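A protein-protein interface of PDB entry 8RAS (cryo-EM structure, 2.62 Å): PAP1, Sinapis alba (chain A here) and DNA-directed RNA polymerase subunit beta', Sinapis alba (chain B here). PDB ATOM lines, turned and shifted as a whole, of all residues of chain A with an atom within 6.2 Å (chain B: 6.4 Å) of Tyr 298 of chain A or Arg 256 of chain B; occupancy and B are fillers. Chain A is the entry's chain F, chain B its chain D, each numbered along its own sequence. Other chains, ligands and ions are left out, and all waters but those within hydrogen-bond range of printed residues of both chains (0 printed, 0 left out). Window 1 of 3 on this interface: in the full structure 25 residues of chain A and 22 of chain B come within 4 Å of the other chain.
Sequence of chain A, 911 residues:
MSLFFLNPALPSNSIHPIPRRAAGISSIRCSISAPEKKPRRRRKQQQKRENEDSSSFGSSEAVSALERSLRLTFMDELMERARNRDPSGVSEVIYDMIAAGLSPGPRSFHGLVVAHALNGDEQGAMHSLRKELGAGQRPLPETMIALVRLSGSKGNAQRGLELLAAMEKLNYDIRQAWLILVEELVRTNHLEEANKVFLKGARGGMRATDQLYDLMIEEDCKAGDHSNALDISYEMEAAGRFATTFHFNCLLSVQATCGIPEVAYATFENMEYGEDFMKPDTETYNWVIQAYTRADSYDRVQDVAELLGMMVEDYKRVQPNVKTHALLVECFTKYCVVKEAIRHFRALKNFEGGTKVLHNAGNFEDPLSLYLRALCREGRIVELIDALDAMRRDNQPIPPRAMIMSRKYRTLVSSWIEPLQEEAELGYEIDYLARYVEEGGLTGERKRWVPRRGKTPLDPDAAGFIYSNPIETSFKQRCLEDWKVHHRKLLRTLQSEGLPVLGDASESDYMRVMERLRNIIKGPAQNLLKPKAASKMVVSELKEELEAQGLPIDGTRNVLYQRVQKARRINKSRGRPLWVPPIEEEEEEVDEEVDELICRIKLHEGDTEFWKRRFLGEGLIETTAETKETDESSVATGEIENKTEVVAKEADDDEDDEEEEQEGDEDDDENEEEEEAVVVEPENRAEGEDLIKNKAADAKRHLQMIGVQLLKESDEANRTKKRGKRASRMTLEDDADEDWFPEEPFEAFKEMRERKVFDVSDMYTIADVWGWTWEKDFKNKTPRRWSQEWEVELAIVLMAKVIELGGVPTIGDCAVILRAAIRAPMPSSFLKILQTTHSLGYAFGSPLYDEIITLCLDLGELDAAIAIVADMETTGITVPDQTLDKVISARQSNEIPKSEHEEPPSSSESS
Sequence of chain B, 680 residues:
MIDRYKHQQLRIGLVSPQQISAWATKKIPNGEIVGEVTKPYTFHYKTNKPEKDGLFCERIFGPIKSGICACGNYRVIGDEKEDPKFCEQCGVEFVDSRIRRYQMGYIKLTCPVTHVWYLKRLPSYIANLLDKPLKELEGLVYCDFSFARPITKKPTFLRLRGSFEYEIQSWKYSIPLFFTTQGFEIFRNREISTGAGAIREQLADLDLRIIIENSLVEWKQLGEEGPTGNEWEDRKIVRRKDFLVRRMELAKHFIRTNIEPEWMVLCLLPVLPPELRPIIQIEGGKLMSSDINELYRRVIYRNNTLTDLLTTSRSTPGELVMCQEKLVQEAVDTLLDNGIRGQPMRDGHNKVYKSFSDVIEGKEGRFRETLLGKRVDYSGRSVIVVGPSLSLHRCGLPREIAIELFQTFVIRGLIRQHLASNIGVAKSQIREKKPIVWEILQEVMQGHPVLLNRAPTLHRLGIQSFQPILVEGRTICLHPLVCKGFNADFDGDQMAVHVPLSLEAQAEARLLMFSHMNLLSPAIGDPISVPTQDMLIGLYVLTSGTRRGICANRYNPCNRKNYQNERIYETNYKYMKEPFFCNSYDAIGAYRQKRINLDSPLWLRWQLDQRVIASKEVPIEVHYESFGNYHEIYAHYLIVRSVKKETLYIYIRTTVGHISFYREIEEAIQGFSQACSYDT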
ATOM      1  N   ALA A 295      11.836   3.483   1.204  1.00  0.00           N
ATOM      2  CA  ALA A 295      12.683   3.053   0.104  1.00  0.00           C
ATOM      3  C   ALA A 295      13.642   4.166  -0.308  1.00  0.00           C
ATOM      4  O   ALA A 295      13.398   5.354  -0.082  1.00  0.00           O
ATOM      5  CB  ALA A 295      11.834   2.627  -1.090  1.00  0.00           C
ATOM      6  N   ASP A 296      14.754   3.761  -0.925  1.00  0.00           N
ATOM      7  CA  ASP A 296      15.769   4.727  -1.332  1.00  0.00           C
ATOM      8  C   ASP A 296      15.325   5.537  -2.545  1.00  0.00           C
ATOM      9  O   ASP A 296      15.488   6.761  -2.571  1.00  0.00           O
ATOM     10  CB  ASP A 296      17.085   4.008  -1.622  1.00  0.00           C
ATOM     11  CG  ASP A 296      17.778   3.535  -0.363  1.00  0.00           C
ATOM     12  OD1 ASP A 296      17.274   3.831   0.740  1.00  0.00           O
ATOM     13  OD2 ASP A 296      18.827   2.868  -0.475  1.00  0.00           O
ATOM     14  N   SER A 297      14.765   4.878  -3.558  1.00  0.00           N
ATOM     15  CA  SER A 297      14.374   5.563  -4.782  1.00  0.00           C
ATOM     16  C   SER A 297      13.104   4.931  -5.331  1.00  0.00           C
ATOM     17  O   SER A 297      12.591   3.946  -4.794  1.00  0.00           O
ATOM     18  CB  SER A 297      15.496   5.527  -5.823  1.00  0.00           C
ATOM     19  OG  SER A 297      14.969   5.468  -7.137  1.00  0.00           O
ATOM     20  N   TYR A 298      12.597   5.526  -6.416  1.00  0.00           N
ATOM     21  CA  TYR A 298      11.351   5.137  -7.074  1.00  0.00           C
ATOM     22  C   TYR A 298      10.151   5.352  -6.157  1.00  0.00           C
ATOM     23  O   TYR A 298      10.308   5.504  -4.942  1.00  0.00           O
ATOM     24  CB  TYR A 298      11.409   3.681  -7.546  1.00  0.00           C
ATOM     25  CG  TYR A 298      12.616   3.359  -8.395  1.00  0.00           C
ATOM     26  CD1 TYR A 298      12.636   3.656  -9.750  1.00  0.00           C
ATOM     27  CD2 TYR A 298      13.733   2.749  -7.842  1.00  0.00           C
ATOM     28  CE1 TYR A 298      13.738   3.362 -10.528  1.00  0.00           C
ATOM     29  CE2 TYR A 298      14.838   2.455  -8.610  1.00  0.00           C
ATOM     30  CZ  TYR A 298      14.835   2.762  -9.953  1.00  0.00           C
ATOM     31  OH  TYR A 298      15.935   2.467 -10.722  1.00  0.00           O
ATOM     32  N   ASP A 299       8.948   5.380  -6.723  1.00  0.00           N
ATOM     33  CA  ASP A 299       7.750   5.559  -5.919  1.00  0.00           C
ATOM     34  C   ASP A 299       7.193   4.214  -5.467  1.00  0.00           C
ATOM     35  O   ASP A 299       7.351   3.197  -6.149  1.00  0.00           O
ATOM     36  CB  ASP A 299       6.707   6.413  -6.664  1.00  0.00           C
ATOM     37  CG  ASP A 299       5.806   5.626  -7.623  1.00  0.00           C
ATOM     38  OD1 ASP A 299       4.874   6.258  -8.163  1.00  0.00           O
ATOM     39  OD2 ASP A 299       6.040   4.441  -7.927  1.00  0.00           O
ATOM     40  N   ARG A 300       6.606   4.203  -4.269  1.00  0.00           N
ATOM     41  CA  ARG A 300       6.071   2.983  -3.679  1.00  0.00           C
ATOM     42  C   ARG A 300       4.673   3.192  -3.110  1.00  0.00           C
ATOM     43  O   ARG A 300       4.220   2.390  -2.289  1.00  0.00           O
ATOM     44  CB  ARG A 300       7.003   2.448  -2.588  1.00  0.00           C
ATOM     45  CG  ARG A 300       8.482   2.650  -2.863  1.00  0.00           C
ATOM     46  CD  ARG A 300       9.001   1.621  -3.848  1.00  0.00           C
ATOM     47  NE  ARG A 300      10.429   1.771  -4.099  1.00  0.00           N
ATOM     48  CZ  ARG A 300      11.190   0.842  -4.659  1.00  0.00           C
ATOM     49  NH1 ARG A 300      10.693  -0.321  -5.040  1.00  0.00           N
ATOM     50  NH2 ARG A 300      12.484   1.089  -4.843  1.00  0.00           N
ATOM     51  N   TYR A 335       3.929  11.206   0.115  1.00  0.00           N
ATOM     52  CA  TYR A 335       3.447  11.205  -1.260  1.00  0.00           C
ATOM     53  C   TYR A 335       2.285  12.165  -1.473  1.00  0.00           C
ATOM     54  O   TYR A 335       1.670  12.148  -2.543  1.00  0.00           O
ATOM     55  CB  TYR A 335       3.044   9.791  -1.676  1.00  0.00           C
ATOM     56  CG  TYR A 335       4.222   8.877  -1.917  1.00  0.00           C
ATOM     57  CD1 TYR A 335       4.878   8.267  -0.859  1.00  0.00           C
ATOM     58  CD2 TYR A 335       4.682   8.630  -3.201  1.00  0.00           C
ATOM     59  CE1 TYR A 335       5.955   7.436  -1.072  1.00  0.00           C
ATOM     60  CE2 TYR A 335       5.760   7.799  -3.424  1.00  0.00           C
ATOM     61  CZ  TYR A 335       6.392   7.206  -2.355  1.00  0.00           C
ATOM     62  OH  TYR A 335       7.466   6.376  -2.568  1.00  0.00           O
ATOM     63  N   LYS A 455      17.974  18.693  -9.216  1.00  0.00           N
ATOM     64  CA  LYS A 455      16.678  18.191  -8.766  1.00  0.00           C
ATOM     65  C   LYS A 455      16.567  18.207  -7.244  1.00  0.00           C
ATOM     66  O   LYS A 455      16.267  17.199  -6.605  1.00  0.00           O
ATOM     67  CB  LYS A 455      16.442  16.791  -9.320  1.00  0.00           C
ATOM     68  CG  LYS A 455      17.613  15.841  -9.135  1.00  0.00           C
ATOM     69  CD  LYS A 455      17.273  14.456  -9.651  1.00  0.00           C
ATOM     70  CE  LYS A 455      17.276  14.428 -11.167  1.00  0.00           C
ATOM     71  NZ  LYS A 455      17.144  13.042 -11.685  1.00  0.00           N
ATOM     72  N   ILE A 466       8.230  13.420  -1.099  1.00  0.00           N
ATOM     73  CA  ILE A 466       8.795  12.730  -2.254  1.00  0.00           C
ATOM     74  C   ILE A 466       8.922  13.681  -3.438  1.00  0.00           C
ATOM     75  O   ILE A 466       9.962  13.737  -4.103  1.00  0.00           O
ATOM     76  CB  ILE A 466       7.942  11.499  -2.605  1.00  0.00           C
ATOM     77  CG1 ILE A 466       7.902  10.527  -1.426  1.00  0.00           C
ATOM     78  CG2 ILE A 466       8.486  10.809  -3.834  1.00  0.00           C
ATOM     79  CD1 ILE A 466       9.247   9.953  -1.063  1.00  0.00           C
ATOM     80  N   TYR A 467       7.871  14.451  -3.712  1.00  0.00           N
ATOM     81  CA  TYR A 467       7.820  15.388  -4.832  1.00  0.00           C
ATOM     82  C   TYR A 467       7.448  16.777  -4.337  1.00  0.00           C
ATOM     83  O   TYR A 467       6.529  17.421  -4.845  1.00  0.00           O
ATOM     84  CB  TYR A 467       6.835  14.932  -5.903  1.00  0.00           C
ATOM     85  CG  TYR A 467       7.006  13.499  -6.347  1.00  0.00           C
ATOM     86  CD1 TYR A 467       8.105  13.112  -7.100  1.00  0.00           C
ATOM     87  CD2 TYR A 467       6.059  12.537  -6.028  1.00  0.00           C
ATOM     88  CE1 TYR A 467       8.260  11.808  -7.514  1.00  0.00           C
ATOM     89  CE2 TYR A 467       6.205  11.229  -6.439  1.00  0.00           C
ATOM     90  CZ  TYR A 467       7.309  10.870  -7.179  1.00  0.00           C
ATOM     91  OH  TYR A 467       7.460   9.566  -7.591  1.00  0.00           O
ATOM     92  N   ARG B  11      19.698  -2.941 -14.567  1.00  0.00           N
ATOM     93  CA  ARG B  11      18.975  -1.719 -14.878  1.00  0.00           C
ATOM     94  C   ARG B  11      19.682  -0.950 -15.981  1.00  0.00           C
ATOM     95  O   ARG B  11      20.890  -0.707 -15.907  1.00  0.00           O
ATOM     96  CB  ARG B  11      18.817  -0.832 -13.638  1.00  0.00           C
ATOM     97  CG  ARG B  11      20.098  -0.561 -12.871  1.00  0.00           C
ATOM     98  CD  ARG B  11      19.934   0.665 -11.993  1.00  0.00           C
ATOM     99  NE  ARG B  11      20.250   1.888 -12.719  1.00  0.00           N
ATOM    100  CZ  ARG B  11      19.808   3.093 -12.390  1.00  0.00           C
ATOM    101  NH1 ARG B  11      18.997   3.274 -11.361  1.00  0.00           N
ATOM    102  NH2 ARG B  11      20.185   4.143 -13.114  1.00  0.00           N
ATOM    103  N   ILE B  12      18.920  -0.575 -17.000  1.00  0.00           N
ATOM    104  CA  ILE B  12      19.355   0.440 -17.946  1.00  0.00           C
ATOM    105  C   ILE B  12      19.182   1.839 -17.356  1.00  0.00           C
ATOM    106  O   ILE B  12      18.486   2.046 -16.359  1.00  0.00           O
ATOM    107  CB  ILE B  12      18.630   0.277 -19.299  1.00  0.00           C
ATOM    108  CG1 ILE B  12      17.109   0.110 -19.135  1.00  0.00           C
ATOM    109  CG2 ILE B  12      19.215  -0.863 -20.100  1.00  0.00           C
ATOM    110  CD1 ILE B  12      16.366   1.135 -18.370  1.00  0.00           C
ATOM    111  N   ALA B 251       7.907  14.042 -15.837  1.00  0.00           N
ATOM    112  CA  ALA B 251       8.664  14.848 -14.887  1.00  0.00           C
ATOM    113  C   ALA B 251       8.806  14.162 -13.537  1.00  0.00           C
ATOM    114  O   ALA B 251       9.814  14.359 -12.851  1.00  0.00           O
ATOM    115  CB  ALA B 251       8.001  16.213 -14.710  1.00  0.00           C
ATOM    116  N   LYS B 252       7.811  13.365 -13.137  1.00  0.00           N
ATOM    117  CA  LYS B 252       7.888  12.667 -11.858  1.00  0.00           C
ATOM    118  C   LYS B 252       9.027  11.657 -11.845  1.00  0.00           C
ATOM    119  O   LYS B 252       9.727  11.513 -10.836  1.00  0.00           O
ATOM    120  CB  LYS B 252       6.560  11.975 -11.560  1.00  0.00           C
ATOM    121  CG  LYS B 252       5.714  12.678 -10.516  1.00  0.00           C
ATOM    122  CD  LYS B 252       4.596  11.777 -10.028  1.00  0.00           C
ATOM    123  CE  LYS B 252       3.565  12.558  -9.235  1.00  0.00           C
ATOM    124  NZ  LYS B 252       2.466  11.683  -8.746  1.00  0.00           N
ATOM    125  N   HIS B 253       9.225  10.943 -12.955  1.00  0.00           N
ATOM    126  CA  HIS B 253      10.241   9.897 -12.991  1.00  0.00           C
ATOM    127  C   HIS B 253      11.648  10.463 -12.866  1.00  0.00           C
ATOM    128  O   HIS B 253      12.540   9.784 -12.349  1.00  0.00           O
ATOM    129  CB  HIS B 253      10.111   9.086 -14.279  1.00  0.00           C
ATOM    130  CG  HIS B 253       9.029   8.054 -14.235  1.00  0.00           C
ATOM    131  ND1 HIS B 253       7.827   8.210 -14.891  1.00  0.00           N
ATOM    132  CD2 HIS B 253       8.965   6.856 -13.612  1.00  0.00           C
ATOM    133  CE1 HIS B 253       7.070   7.149 -14.675  1.00  0.00           C
ATOM    134  NE2 HIS B 253       7.738   6.313 -13.902  1.00  0.00           N
ATOM    135  N   PHE B 254      11.872  11.692 -13.337  1.00  0.00           N
ATOM    136  CA  PHE B 254      13.198  12.286 -13.220  1.00  0.00           C
ATOM    137  C   PHE B 254      13.546  12.608 -11.773  1.00  0.00           C
ATOM    138  O   PHE B 254      14.717  12.526 -11.388  1.00  0.00           O
ATOM    139  CB  PHE B 254      13.292  13.545 -14.079  1.00  0.00           C
ATOM    140  CG  PHE B 254      13.482  13.267 -15.540  1.00  0.00           C
ATOM    141  CD1 PHE B 254      14.673  12.745 -16.009  1.00  0.00           C
ATOM    142  CD2 PHE B 254      12.468  13.524 -16.445  1.00  0.00           C
ATOM    143  CE1 PHE B 254      14.850  12.487 -17.351  1.00  0.00           C
ATOM    144  CE2 PHE B 254      12.639  13.267 -17.788  1.00  0.00           C
ATOM    145  CZ  PHE B 254      13.832  12.749 -18.241  1.00  0.00           C
ATOM    146  N   ILE B 255      12.553  12.979 -10.963  1.00  0.00           N
ATOM    147  CA  ILE B 255      12.826  13.365  -9.582  1.00  0.00           C
ATOM    148  C   ILE B 255      13.324  12.175  -8.772  1.00  0.00           C
ATOM    149  O   ILE B 255      14.291  12.290  -8.010  1.00  0.00           O
ATOM    150  CB  ILE B 255      11.574  13.993  -8.946  1.00  0.00           C
ATOM    151  CG1 ILE B 255      10.961  15.030  -9.888  1.00  0.00           C
ATOM    152  CG2 ILE B 255      11.918  14.613  -7.604  1.00  0.00           C
ATOM    153  CD1 ILE B 255       9.958  15.937  -9.223  1.00  0.00           C
ATOM    154  N   ARG B 256      12.678  11.019  -8.918  1.00  0.00           N
ATOM    155  CA  ARG B 256      13.008   9.870  -8.086  1.00  0.00           C
ATOM    156  C   ARG B 256      14.240   9.113  -8.558  1.00  0.00           C
ATOM    157  O   ARG B 256      14.773   8.301  -7.796  1.00  0.00           O
ATOM    158  CB  ARG B 256      11.818   8.914  -8.017  1.00  0.00           C
ATOM    159  CG  ARG B 256      10.733   9.372  -7.067  1.00  0.00           C
ATOM    160  CD  ARG B 256      11.292   9.586  -5.674  1.00  0.00           C
ATOM    161  NE  ARG B 256      11.049   8.442  -4.803  1.00  0.00           N
ATOM    162  CZ  ARG B 256      11.716   8.200  -3.682  1.00  0.00           C
ATOM    163  NH1 ARG B 256      12.677   9.004  -3.263  1.00  0.00           N
ATOM    164  NH2 ARG B 256      11.407   7.125  -2.964  1.00  0.00           N
ATOM    165  N   THR B 257      14.704   9.350  -9.779  1.00  0.00           N
ATOM    166  CA  THR B 257      15.870   8.662 -10.304  1.00  0.00           C
ATOM    167  C   THR B 257      17.081   9.590 -10.291  1.00  0.00           C
ATOM    168  O   THR B 257      17.004  10.759  -9.907  1.00  0.00           O
ATOM    169  CB  THR B 257      15.594   8.144 -11.716  1.00  0.00           C
ATOM    170  OG1 THR B 257      14.748   9.068 -12.409  1.00  0.00           O
ATOM    171  CG2 THR B 257      14.911   6.794 -11.654  1.00  0.00           C
ATOM    172  N   ASN B 258      18.220   9.052 -10.719  1.00  0.00           N
ATOM    173  CA  ASN B 258      19.445   9.823 -10.862  1.00  0.00           C
ATOM    174  C   ASN B 258      19.642  10.337 -12.281  1.00  0.00           C
ATOM    175  O   ASN B 258      20.690  10.916 -12.582  1.00  0.00           O
ATOM    176  CB  ASN B 258      20.651   8.983 -10.437  1.00  0.00           C
ATOM    177  CG  ASN B 258      20.491   7.521 -10.788  1.00  0.00           C
ATOM    178  OD1 ASN B 258      19.716   6.801 -10.160  1.00  0.00           O
ATOM    179  ND2 ASN B 258      21.229   7.072 -11.795  1.00  0.00           N
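The backbone carbonyl oxygen (O) of Arg 256 of chain B sits at hydrogen-bond distance from the side-chain hydroxyl (OG) of Ser 297 of chain A (2.9 Å). O of Thr 257 of chain B is in hydrogen-bond range of NZ of Lys 455 of chain A (2.9 Å). OH of Tyr 298 of chain A sits at hydrogen-bond distance from NH1 of Arg 11 of chain B (3.2 Å). O of Phe 254 of chain B is in hydrogen-bond range of NZ of Lys 455 of chain A, at 2.5 Å. The guanidinium group (NH2) of Arg 256 of chain B sits at hydrogen-bond distance from the backbone carbonyl oxygen (O) of Tyr 298 of chain A.
The guanidinium group (NH2) of Arg 11 of chain B lies close to the side-chain amide nitrogen (ND2) of Asn 258 of chain B (3.4 Å). O of Ser 297 of chain A is in hydrogen-bond range of NH2 of Arg 300 of chain A (2.9 Å).
Among the printed residues, merely in contact across the chains: Ala 295 of chain A with Arg 256 of chain B (3.9 Å), Asp 296 of chain A with Arg 256 of chain B (3.7 Å), Tyr 298 of chain A with Thr 257 of chain B (3.8 Å), Lys 455 of chain A with Asn 258 of chain B (3.7 Å), Ile 466 of chain A with Arg 256 of chain B (3.6 Å), Tyr 467 of chain A with Lys 252 of chain B (3.6 Å), Tyr 467 of chain A with Ile 255 of chain B (3.99 Å) and Tyr 467 of chain A with Arg 256 of chain B (3.3 Å).
Tyr 298 of chain A touches three residues of chain B. Of chain A, only Ala 295, Asp 296, Ser 297, Tyr 298, Ile 466 and Tyr 467 come within 4 Å of Arg 256 of chain B. Of the printed residues of chain A, Asn 258 of chain B touches Lys 455. Of the printed residues of chain B, Ala 295 of chain A touches Arg 256 (3.9 Å). Of the printed residues of chain B, Tyr 467 of chain A touches Lys 252, Ile 255 and Arg 256. Printed residues of chain B within 4 Å of Lys 455 of chain A: Phe 254, Thr 257 and Asn 258. The nearest printed residue of chain A that does not touch Asn 258 of chain B is Tyr 298 of chain A (5.8 Å).
Hydrophobic or aromatic side chains of chain A within 4 Å of the printed part of chain B: Tyr 298, Ile 466 and Tyr 467. Of the 10 printed residues of chain B, 7 touch a printed residue of chain A. Among the printed residues, 13 pairs touch across the chains. Among the printed residues, no Asp or Glu carboxylate lies within 4 Å of a Lys or Arg side-chain nitrogen of the other chain.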
